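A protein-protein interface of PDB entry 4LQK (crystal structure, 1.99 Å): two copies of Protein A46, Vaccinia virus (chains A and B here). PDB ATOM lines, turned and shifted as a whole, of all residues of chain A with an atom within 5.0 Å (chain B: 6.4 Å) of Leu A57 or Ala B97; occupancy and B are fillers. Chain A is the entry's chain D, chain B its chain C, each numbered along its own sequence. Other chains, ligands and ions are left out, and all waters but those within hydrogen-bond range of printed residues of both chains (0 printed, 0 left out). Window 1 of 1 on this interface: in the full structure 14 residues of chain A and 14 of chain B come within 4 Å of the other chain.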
ATOM      1  N   VAL A  51     -21.218  13.180  -3.428  1.00  0.00           N
ATOM      2  CA  VAL A  51     -20.240  13.442  -4.481  1.00  0.00           C
ATOM      3  C   VAL A  51     -20.105  12.294  -5.484  1.00  0.00           C
ATOM      4  O   VAL A  51     -19.602  12.507  -6.586  1.00  0.00           O
ATOM      5  CB  VAL A  51     -18.849  13.839  -3.929  1.00  0.00           C
ATOM      6  CG1 VAL A  51     -18.946  15.149  -3.162  1.00  0.00           C
ATOM      7  CG2 VAL A  51     -18.257  12.743  -3.055  1.00  0.00           C
ATOM      8  N   SER A  55     -24.165  13.928 -10.696  1.00  0.00           N
ATOM      9  CA  SER A  55     -23.975  15.374 -10.683  1.00  0.00           C
ATOM     10  C   SER A  55     -22.987  15.840  -9.589  1.00  0.00           C
ATOM     11  O   SER A  55     -22.851  17.040  -9.338  1.00  0.00           O
ATOM     12  CB  SER A  55     -25.335  16.069 -10.513  1.00  0.00           C
ATOM     13  OG  SER A  55     -26.040  16.047 -11.740  1.00  0.00           O
ATOM     14  N   GLY A  56     -22.290  14.896  -8.966  1.00  0.00           N
ATOM     15  CA  GLY A  56     -21.376  15.183  -7.843  1.00  0.00           C
ATOM     16  C   GLY A  56     -20.361  16.268  -8.104  1.00  0.00           C
ATOM     17  O   GLY A  56     -20.067  17.082  -7.230  1.00  0.00           O
ATOM     18  N   LEU A  57     -19.830  16.287  -9.322  1.00  0.00           N
ATOM     19  CA  LEU A  57     -18.866  17.293  -9.733  1.00  0.00           C
ATOM     20  C   LEU A  57     -19.472  18.685  -9.616  1.00  0.00           C
ATOM     21  O   LEU A  57     -18.894  19.569  -8.973  1.00  0.00           O
ATOM     22  CB  LEU A  57     -18.412  17.053 -11.164  1.00  0.00           C
ATOM     23  CG  LEU A  57     -17.461  18.094 -11.745  1.00  0.00           C
ATOM     24  CD1 LEU A  57     -16.242  18.277 -10.847  1.00  0.00           C
ATOM     25  CD2 LEU A  57     -17.047  17.693 -13.151  1.00  0.00           C
ATOM     26  N   PHE A  58     -20.639  18.856 -10.235  1.00  0.00           N
ATOM     27  CA  PHE A  58     -21.293  20.155 -10.305  1.00  0.00           C
ATOM     28  C   PHE A  58     -21.883  20.565  -8.966  1.00  0.00           C
ATOM     29  O   PHE A  58     -21.859  21.736  -8.636  1.00  0.00           O
ATOM     30  CB  PHE A  58     -22.313  20.183 -11.453  1.00  0.00           C
ATOM     31  CG  PHE A  58     -21.671  20.019 -12.806  1.00  0.00           C
ATOM     32  CD1 PHE A  58     -21.211  21.113 -13.504  1.00  0.00           C
ATOM     33  CD2 PHE A  58     -21.446  18.756 -13.333  1.00  0.00           C
ATOM     34  CE1 PHE A  58     -20.575  20.967 -14.731  1.00  0.00           C
ATOM     35  CE2 PHE A  58     -20.800  18.595 -14.553  1.00  0.00           C
ATOM     36  CZ  PHE A  58     -20.365  19.705 -15.254  1.00  0.00           C
ATOM     37  N   ASP A  59     -22.384  19.603  -8.190  1.00  0.00           N
ATOM     38  CA  ASP A  59     -22.857  19.872  -6.832  1.00  0.00           C
ATOM     39  C   ASP A  59     -21.719  20.247  -5.873  1.00  0.00           C
ATOM     40  O   ASP A  59     -21.918  21.012  -4.916  1.00  0.00           O
ATOM     41  CB  ASP A  59     -23.613  18.665  -6.264  1.00  0.00           C
ATOM     42  CG  ASP A  59     -24.939  18.397  -6.986  1.00  0.00           C
ATOM     43  OD1 ASP A  59     -25.421  19.284  -7.702  1.00  0.00           O
ATOM     44  OD2 ASP A  59     -25.481  17.273  -6.859  1.00  0.00           O
ATOM     45  N   PHE A  60     -20.533  19.691  -6.097  1.00  0.00           N
ATOM     46  CA  PHE A  60     -19.383  20.064  -5.286  1.00  0.00           C
ATOM     47  C   PHE A  60     -18.963  21.484  -5.614  1.00  0.00           C
ATOM     48  O   PHE A  60     -18.740  22.290  -4.710  1.00  0.00           O
ATOM     49  CB  PHE A  60     -18.184  19.142  -5.520  1.00  0.00           C
ATOM     50  CG  PHE A  60     -16.967  19.580  -4.777  1.00  0.00           C
ATOM     51  CD1 PHE A  60     -16.780  19.197  -3.459  1.00  0.00           C
ATOM     52  CD2 PHE A  60     -16.048  20.436  -5.365  1.00  0.00           C
ATOM     53  CE1 PHE A  60     -15.675  19.623  -2.742  1.00  0.00           C
ATOM     54  CE2 PHE A  60     -14.933  20.864  -4.654  1.00  0.00           C
ATOM     55  CZ  PHE A  60     -14.757  20.457  -3.339  1.00  0.00           C
ATOM     56  N   VAL A  61     -18.798  21.771  -6.903  1.00  0.00           N
ATOM     57  CA  VAL A  61     -18.397  23.106  -7.343  1.00  0.00           C
ATOM     58  C   VAL A  61     -19.400  24.166  -6.865  1.00  0.00           C
ATOM     59  O   VAL A  61     -19.000  25.261  -6.467  1.00  0.00           O
ATOM     60  CB  VAL A  61     -18.212  23.173  -8.872  1.00  0.00           C
ATOM     61  CG1 VAL A  61     -18.104  24.621  -9.361  1.00  0.00           C
ATOM     62  CG2 VAL A  61     -16.969  22.380  -9.269  1.00  0.00           C
ATOM     63  N   TRP A  86     -12.485  10.874  -5.642  1.00  0.00           N
ATOM     64  CA  TRP A  86     -12.906  10.483  -6.982  1.00  0.00           C
ATOM     65  C   TRP A  86     -11.858   9.632  -7.689  1.00  0.00           C
ATOM     66  O   TRP A  86     -12.195   8.763  -8.494  1.00  0.00           O
ATOM     67  CB  TRP A  86     -13.228  11.702  -7.858  1.00  0.00           C
ATOM     68  CG  TRP A  86     -14.554  12.341  -7.551  1.00  0.00           C
ATOM     69  CD1 TRP A  86     -15.686  11.713  -7.153  1.00  0.00           C
ATOM     70  CD2 TRP A  86     -14.872  13.731  -7.638  1.00  0.00           C
ATOM     71  NE1 TRP A  86     -16.701  12.619  -6.971  1.00  0.00           N
ATOM     72  CE2 TRP A  86     -16.224  13.872  -7.262  1.00  0.00           C
ATOM     73  CE3 TRP A  86     -14.150  14.871  -8.013  1.00  0.00           C
ATOM     74  CZ2 TRP A  86     -16.861  15.104  -7.228  1.00  0.00           C
ATOM     75  CZ3 TRP A  86     -14.791  16.104  -7.983  1.00  0.00           C
ATOM     76  CH2 TRP A  86     -16.125  16.208  -7.595  1.00  0.00           C
ATOM     77  N   TYR A  93     -11.528  11.345 -14.286  1.00  0.00           N
ATOM     78  CA  TYR A  93     -11.954  12.391 -15.208  1.00  0.00           C
ATOM     79  C   TYR A  93     -12.528  13.615 -14.445  1.00  0.00           C
ATOM     80  O   TYR A  93     -12.336  14.760 -14.859  1.00  0.00           O
ATOM     81  CB  TYR A  93     -12.964  11.819 -16.223  1.00  0.00           C
ATOM     82  CG  TYR A  93     -14.216  11.270 -15.599  1.00  0.00           C
ATOM     83  CD1 TYR A  93     -14.296   9.950 -15.191  1.00  0.00           C
ATOM     84  CD2 TYR A  93     -15.335  12.071 -15.433  1.00  0.00           C
ATOM     85  CE1 TYR A  93     -15.451   9.443 -14.615  1.00  0.00           C
ATOM     86  CE2 TYR A  93     -16.494  11.576 -14.864  1.00  0.00           C
ATOM     87  CZ  TYR A  93     -16.550  10.263 -14.460  1.00  0.00           C
ATOM     88  OH  TYR A  93     -17.701   9.782 -13.883  1.00  0.00           O
ATOM     89  N   ARG A  94     -13.185  13.362 -13.316  1.00  0.00           N
ATOM     90  CA  ARG A  94     -13.674  14.439 -12.438  1.00  0.00           C
ATOM     91  C   ARG A  94     -12.539  15.232 -11.770  1.00  0.00           C
ATOM     92  O   ARG A  94     -12.614  16.446 -11.638  1.00  0.00           O
ATOM     93  CB  ARG A  94     -14.589  13.856 -11.369  1.00  0.00           C
ATOM     94  CG  ARG A  94     -15.915  13.376 -11.935  1.00  0.00           C
ATOM     95  CD  ARG A  94     -16.842  13.016 -10.813  1.00  0.00           C
ATOM     96  NE  ARG A  94     -18.101  12.436 -11.264  1.00  0.00           N
ATOM     97  CZ  ARG A  94     -19.132  12.188 -10.462  1.00  0.00           C
ATOM     98  NH1 ARG A  94     -19.071  12.497  -9.170  1.00  0.00           N
ATOM     99  NH2 ARG A  94     -20.245  11.654 -10.959  1.00  0.00           N
ATOM    100  N   ALA A  97     -11.382  17.694 -14.493  1.00  0.00           N
ATOM    101  CA  ALA A  97     -12.346  18.774 -14.710  1.00  0.00           C
ATOM    102  C   ALA A  97     -12.338  19.767 -13.529  1.00  0.00           C
ATOM    103  O   ALA A  97     -12.311  20.976 -13.731  1.00  0.00           O
ATOM    104  CB  ALA A  97     -13.736  18.211 -14.921  1.00  0.00           C
ATOM    105  N   LEU A  98     -12.321  19.253 -12.306  1.00  0.00           N
ATOM    106  CA  LEU A  98     -12.270  20.105 -11.115  1.00  0.00           C
ATOM    107  C   LEU A  98     -11.013  21.000 -11.024  1.00  0.00           C
ATOM    108  O   LEU A  98     -11.107  22.216 -10.757  1.00  0.00           O
ATOM    109  CB  LEU A  98     -12.384  19.266  -9.844  1.00  0.00           C
ATOM    110  CG  LEU A  98     -12.581  20.081  -8.557  1.00  0.00           C
ATOM    111  CD1 LEU A  98     -13.924  20.790  -8.579  1.00  0.00           C
ATOM    112  CD2 LEU A  98     -12.485  19.223  -7.303  1.00  0.00           C
ATOM    113  N   LEU B  57     -16.140  23.809 -19.448  1.00  0.00           N
ATOM    114  CA  LEU B  57     -17.151  22.834 -19.057  1.00  0.00           C
ATOM    115  C   LEU B  57     -18.236  23.470 -18.201  1.00  0.00           C
ATOM    116  O   LEU B  57     -19.422  23.254 -18.436  1.00  0.00           O
ATOM    117  CB  LEU B  57     -16.527  21.643 -18.309  1.00  0.00           C
ATOM    118  CG  LEU B  57     -17.502  20.645 -17.676  1.00  0.00           C
ATOM    119  CD1 LEU B  57     -18.324  19.914 -18.737  1.00  0.00           C
ATOM    120  CD2 LEU B  57     -16.766  19.633 -16.817  1.00  0.00           C
ATOM    121  N   PHE B  58     -17.816  24.257 -17.224  1.00  0.00           N
ATOM    122  CA  PHE B  58     -18.747  24.897 -16.300  1.00  0.00           C
ATOM    123  C   PHE B  58     -19.501  26.044 -16.947  1.00  0.00           C
ATOM    124  O   PHE B  58     -20.669  26.246 -16.647  1.00  0.00           O
ATOM    125  CB  PHE B  58     -18.023  25.304 -15.014  1.00  0.00           C
ATOM    126  CG  PHE B  58     -17.533  24.123 -14.254  1.00  0.00           C
ATOM    127  CD1 PHE B  58     -16.317  23.544 -14.561  1.00  0.00           C
ATOM    128  CD2 PHE B  58     -18.330  23.532 -13.300  1.00  0.00           C
ATOM    129  CE1 PHE B  58     -15.892  22.418 -13.888  1.00  0.00           C
ATOM    130  CE2 PHE B  58     -17.915  22.403 -12.640  1.00  0.00           C
ATOM    131  CZ  PHE B  58     -16.685  21.848 -12.930  1.00  0.00           C
ATOM    132  N   LYS B  92     -11.256  14.761 -23.492  1.00  0.00           N
ATOM    133  CA  LYS B  92     -12.263  13.718 -23.398  1.00  0.00           C
ATOM    134  C   LYS B  92     -12.842  13.664 -21.982  1.00  0.00           C
ATOM    135  O   LYS B  92     -14.006  13.314 -21.786  1.00  0.00           O
ATOM    136  CB  LYS B  92     -11.667  12.361 -23.804  1.00  0.00           C
ATOM    137  CG  LYS B  92     -12.615  11.179 -23.711  1.00  0.00           C
ATOM    138  CD  LYS B  92     -13.516  11.115 -24.919  1.00  0.00           C
ATOM    139  CE  LYS B  92     -14.580  10.043 -24.779  1.00  0.00           C
ATOM    140  NZ  LYS B  92     -15.591  10.217 -25.859  1.00  0.00           N
ATOM    141  N   TYR B  93     -12.031  14.007 -20.991  1.00  0.00           N
ATOM    142  CA  TYR B  93     -12.516  14.016 -19.612  1.00  0.00           C
ATOM    143  C   TYR B  93     -13.733  14.923 -19.448  1.00  0.00           C
ATOM    144  O   TYR B  93     -14.595  14.634 -18.648  1.00  0.00           O
ATOM    145  CB  TYR B  93     -11.413  14.416 -18.630  1.00  0.00           C
ATOM    146  CG  TYR B  93     -10.784  15.763 -18.873  1.00  0.00           C
ATOM    147  CD1 TYR B  93      -9.731  15.904 -19.761  1.00  0.00           C
ATOM    148  CD2 TYR B  93     -11.223  16.895 -18.188  1.00  0.00           C
ATOM    149  CE1 TYR B  93      -9.144  17.125 -19.982  1.00  0.00           C
ATOM    150  CE2 TYR B  93     -10.625  18.120 -18.390  1.00  0.00           C
ATOM    151  CZ  TYR B  93      -9.590  18.231 -19.292  1.00  0.00           C
ATOM    152  OH  TYR B  93      -8.990  19.452 -19.534  1.00  0.00           O
ATOM    153  N   ARG B  94     -13.790  16.000 -20.212  1.00  0.00           N
ATOM    154  CA  ARG B  94     -14.947  16.921 -20.196  1.00  0.00           C
ATOM    155  C   ARG B  94     -16.186  16.285 -20.811  1.00  0.00           C
ATOM    156  O   ARG B  94     -17.283  16.487 -20.311  1.00  0.00           O
ATOM    157  CB  ARG B  94     -14.637  18.217 -20.938  1.00  0.00           C
ATOM    158  CG  ARG B  94     -13.704  19.150 -20.188  1.00  0.00           C
ATOM    159  CD  ARG B  94     -13.586  20.490 -20.895  1.00  0.00           C
ATOM    160  NE  ARG B  94     -12.543  21.332 -20.292  1.00  0.00           N
ATOM    161  CZ  ARG B  94     -12.265  22.581 -20.661  1.00  0.00           C
ATOM    162  NH1 ARG B  94     -12.937  23.165 -21.643  1.00  0.00           N
ATOM    163  NH2 ARG B  94     -11.291  23.247 -20.065  1.00  0.00           N
ATOM    164  N   CYS B  95     -16.006  15.526 -21.892  1.00  0.00           N
ATOM    165  CA  CYS B  95     -17.083  14.711 -22.470  1.00  0.00           C
ATOM    166  C   CYS B  95     -17.747  13.768 -21.486  1.00  0.00           C
ATOM    167  O   CYS B  95     -18.992  13.592 -21.504  1.00  0.00           O
ATOM    168  CB  CYS B  95     -16.550  13.848 -23.602  1.00  0.00           C
ATOM    169  SG  CYS B  95     -15.574  14.740 -24.794  1.00  0.00           S
ATOM    170  N   MET B  96     -16.911  13.118 -20.671  1.00  0.00           N
ATOM    171  CA  MET B  96     -17.369  12.175 -19.662  1.00  0.00           C
ATOM    172  C   MET B  96     -18.086  12.897 -18.559  1.00  0.00           C
ATOM    173  O   MET B  96     -19.123  12.449 -18.112  1.00  0.00           O
ATOM    174  CB  MET B  96     -16.200  11.363 -19.072  1.00  0.00           C
ATOM    175  CG  MET B  96     -15.567  10.435 -20.126  1.00  0.00           C
ATOM    176  SD  MET B  96     -13.811   9.819 -19.462  1.00  0.00           S
ATOM    177  CE  MET B  96     -14.513   8.431 -18.260  1.00  0.00           C
ATOM    178  N   ALA B  97     -17.521  14.001 -18.083  1.00  0.00           N
ATOM    179  CA  ALA B  97     -18.153  14.786 -17.006  1.00  0.00           C
ATOM    180  C   ALA B  97     -19.474  15.418 -17.489  1.00  0.00           C
ATOM    181  O   ALA B  97     -20.464  15.405 -16.764  1.00  0.00           O
ATOM    182  CB  ALA B  97     -17.204  15.869 -16.511  1.00  0.00           C
ATOM    183  N   LEU B  98     -19.491  15.945 -18.712  1.00  0.00           N
ATOM    184  CA  LEU B  98     -20.720  16.552 -19.251  1.00  0.00           C
ATOM    185  C   LEU B  98     -21.862  15.545 -19.421  1.00  0.00           C
ATOM    186  O   LEU B  98     -23.002  15.813 -19.015  1.00  0.00           O
ATOM    187  CB  LEU B  98     -20.435  17.261 -20.575  1.00  0.00           C
ATOM    188  CG  LEU B  98     -21.643  17.958 -21.198  1.00  0.00           C
ATOM    189  CD1 LEU B  98     -22.085  19.153 -20.347  1.00  0.00           C
ATOM    190  CD2 LEU B  98     -21.331  18.376 -22.615  1.00  0.00           C
ATOM    191  N   ALA B  99     -21.547  14.387 -20.011  1.00  0.00           N
ATOM    192  CA  ALA B  99     -22.533  13.353 -20.331  1.00  0.00           C
ATOM    193  C   ALA B  99     -23.306  12.871 -19.109  1.00  0.00           C
ATOM    194  O   ALA B  99     -24.535  12.758 -19.145  1.00  0.00           O
ATOM    195  CB  ALA B  99     -21.852  12.160 -21.012  1.00  0.00           C
ATOM    196  N   GLU B 100     -22.587  12.564 -18.036  1.00  0.00           N
ATOM    197  CA  GLU B 100     -23.227  12.065 -16.827  1.00  0.00           C
ATOM    198  C   GLU B 100     -24.132  13.122 -16.189  1.00  0.00           C
ATOM    199  O   GLU B 100     -25.210  12.795 -15.696  1.00  0.00           O
ATOM    200  CB  GLU B 100     -22.199  11.552 -15.805  1.00  0.00           C
ATOM    201  CG  GLU B 100     -21.179  12.587 -15.346  1.00  0.00           C
ATOM    202  CD  GLU B 100     -20.112  12.019 -14.412  1.00  0.00           C
ATOM    203  OE1 GLU B 100     -20.221  10.843 -13.990  1.00  0.00           O
ATOM    204  OE2 GLU B 100     -19.167  12.767 -14.081  1.00  0.00           O
ATOM    205  N   HIS B 101     -23.707  14.378 -16.221  1.00  0.00           N
ATOM    206  CA  HIS B 101     -24.476  15.452 -15.577  1.00  0.00           C
ATOM    207  C   HIS B 101     -25.673  15.902 -16.406  1.00  0.00           C
ATOM    208  O   HIS B 101     -26.755  16.093 -15.856  1.00  0.00           O
ATOM    209  CB  HIS B 101     -23.593  16.651 -15.284  1.00  0.00           C
ATOM    210  CG  HIS B 101     -24.319  17.793 -14.646  1.00  0.00           C
ATOM    211  ND1 HIS B 101     -25.005  17.666 -13.459  1.00  0.00           N
ATOM    212  CD2 HIS B 101     -24.442  19.089 -15.012  1.00  0.00           C
ATOM    213  CE1 HIS B 101     -25.517  18.836 -13.116  1.00  0.00           C
ATOM    214  NE2 HIS B 101     -25.199  19.715 -14.048  1.00  0.00           N
ATOM    215  N   ILE B 102     -25.487  16.096 -17.712  1.00  0.00           N
ATOM    216  CA  ILE B 102     -26.629  16.430 -18.586  1.00  0.00           C
ATOM    217  C   ILE B 102     -27.703  15.335 -18.559  1.00  0.00           C
ATOM    218  O   ILE B 102     -28.891  15.627 -18.368  1.00  0.00           O
ATOM    219  CB  ILE B 102     -26.204  16.707 -20.045  1.00  0.00           C
ATOM    220  CG1 ILE B 102     -25.371  17.981 -20.125  1.00  0.00           C
ATOM    221  CG2 ILE B 102     -27.423  16.811 -20.956  1.00  0.00           C
ATOM    222  CD1 ILE B 102     -26.011  19.215 -19.509  1.00  0.00           C
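Printed residues of chain A within 4 Å of Glu B100: Tyr A93 (2.7 Å) and Arg A94 (3.0 Å). Of the printed residues of chain A, Met B96 touches Tyr A93 (3.4 Å). Printed residues of chain B within 4 Å of Arg A94: Glu B100. Of the printed residues of chain B, Ala A97 touches Leu B57 (3.8 Å), Phe B58 (3.9 Å) and Tyr B93 (3.8 Å). The nearest residue of chain A that does not touch Ala B97 is Ala A97 (4.5 Å). The nearest printed residue of chain B that does not touch Tyr A93 is Arg B94 (5.7 Å).
The side-chain carboxylate (OE2) of Glu B100 is in salt-bridge range of the guanidinium group (NE) of Arg A94. The side-chain carboxylate (OE1) of Glu B100 is in hydrogen-bond range of the side-chain hydroxyl (OH) of Tyr A93, at 2.7 Å. The side-chain hydroxyl of Ser A55 lies within hydrogen-bond range of a ring nitrogen (ND1) of His B101 (2.6 Å).
Printed residues of chain B that touch a printed residue of chain A: Leu B57, Phe B58, Tyr B93, Met B96, Ala B97, Glu B100 and His B101. Hydrophobic or aromatic side chains of chain A that line the printed part of chain B: Leu A57, Phe A58, Val A61, Tyr A93 and Ala A97. Among the printed residues, Asp or Glu carboxylates within 4 Å of a Lys or Arg side-chain nitrogen of the other chain: Arg A94 with Glu B100 (3.0 Å).
Leu A57 touches Ala B97, and with the chains exchanged Ala A97 touches Leu B57. Phe A58 touches Leu B57, but with the chains exchanged Leu A57 does not touch Phe B58 (4.01 Å). Phe B58 touches its own counterpart, Phe A58. Tyr B93 touches its own counterpart, Tyr A93. 6 positions are printed for both chains. Of the 15 pairs that touch across the chains among the printed residues, 8 have their exchanged pair printed and touching as well.
O of Val A51 lies within hydrogen-bond range of NH1 of Arg A94, at 2.6 Å.
CD2 of Leu A57 touches CB of Ala B97, 3.8 Å away. Phe A58 touches Leu B57. Phe B58 touches Phe A58 (CE2 to CD1, 3.6 Å). Ala B97 touches Phe A58. His B101 touches Phe A58 (CG to CD2, 3.3 Å). CB of Tyr B93 touches CB of Tyr A93, 3.9 Å away. N of Ala B97 touches CD2 of Tyr A93, at 3.9 Å. Leu B57 touches Ala A97 (CD2 to CB, 3.8 Å). CE1 of Phe B58 touches O of Ala A97 (3.9 Å). Ala A97 touches Tyr B93 (N to CD2, 3.8 Å).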
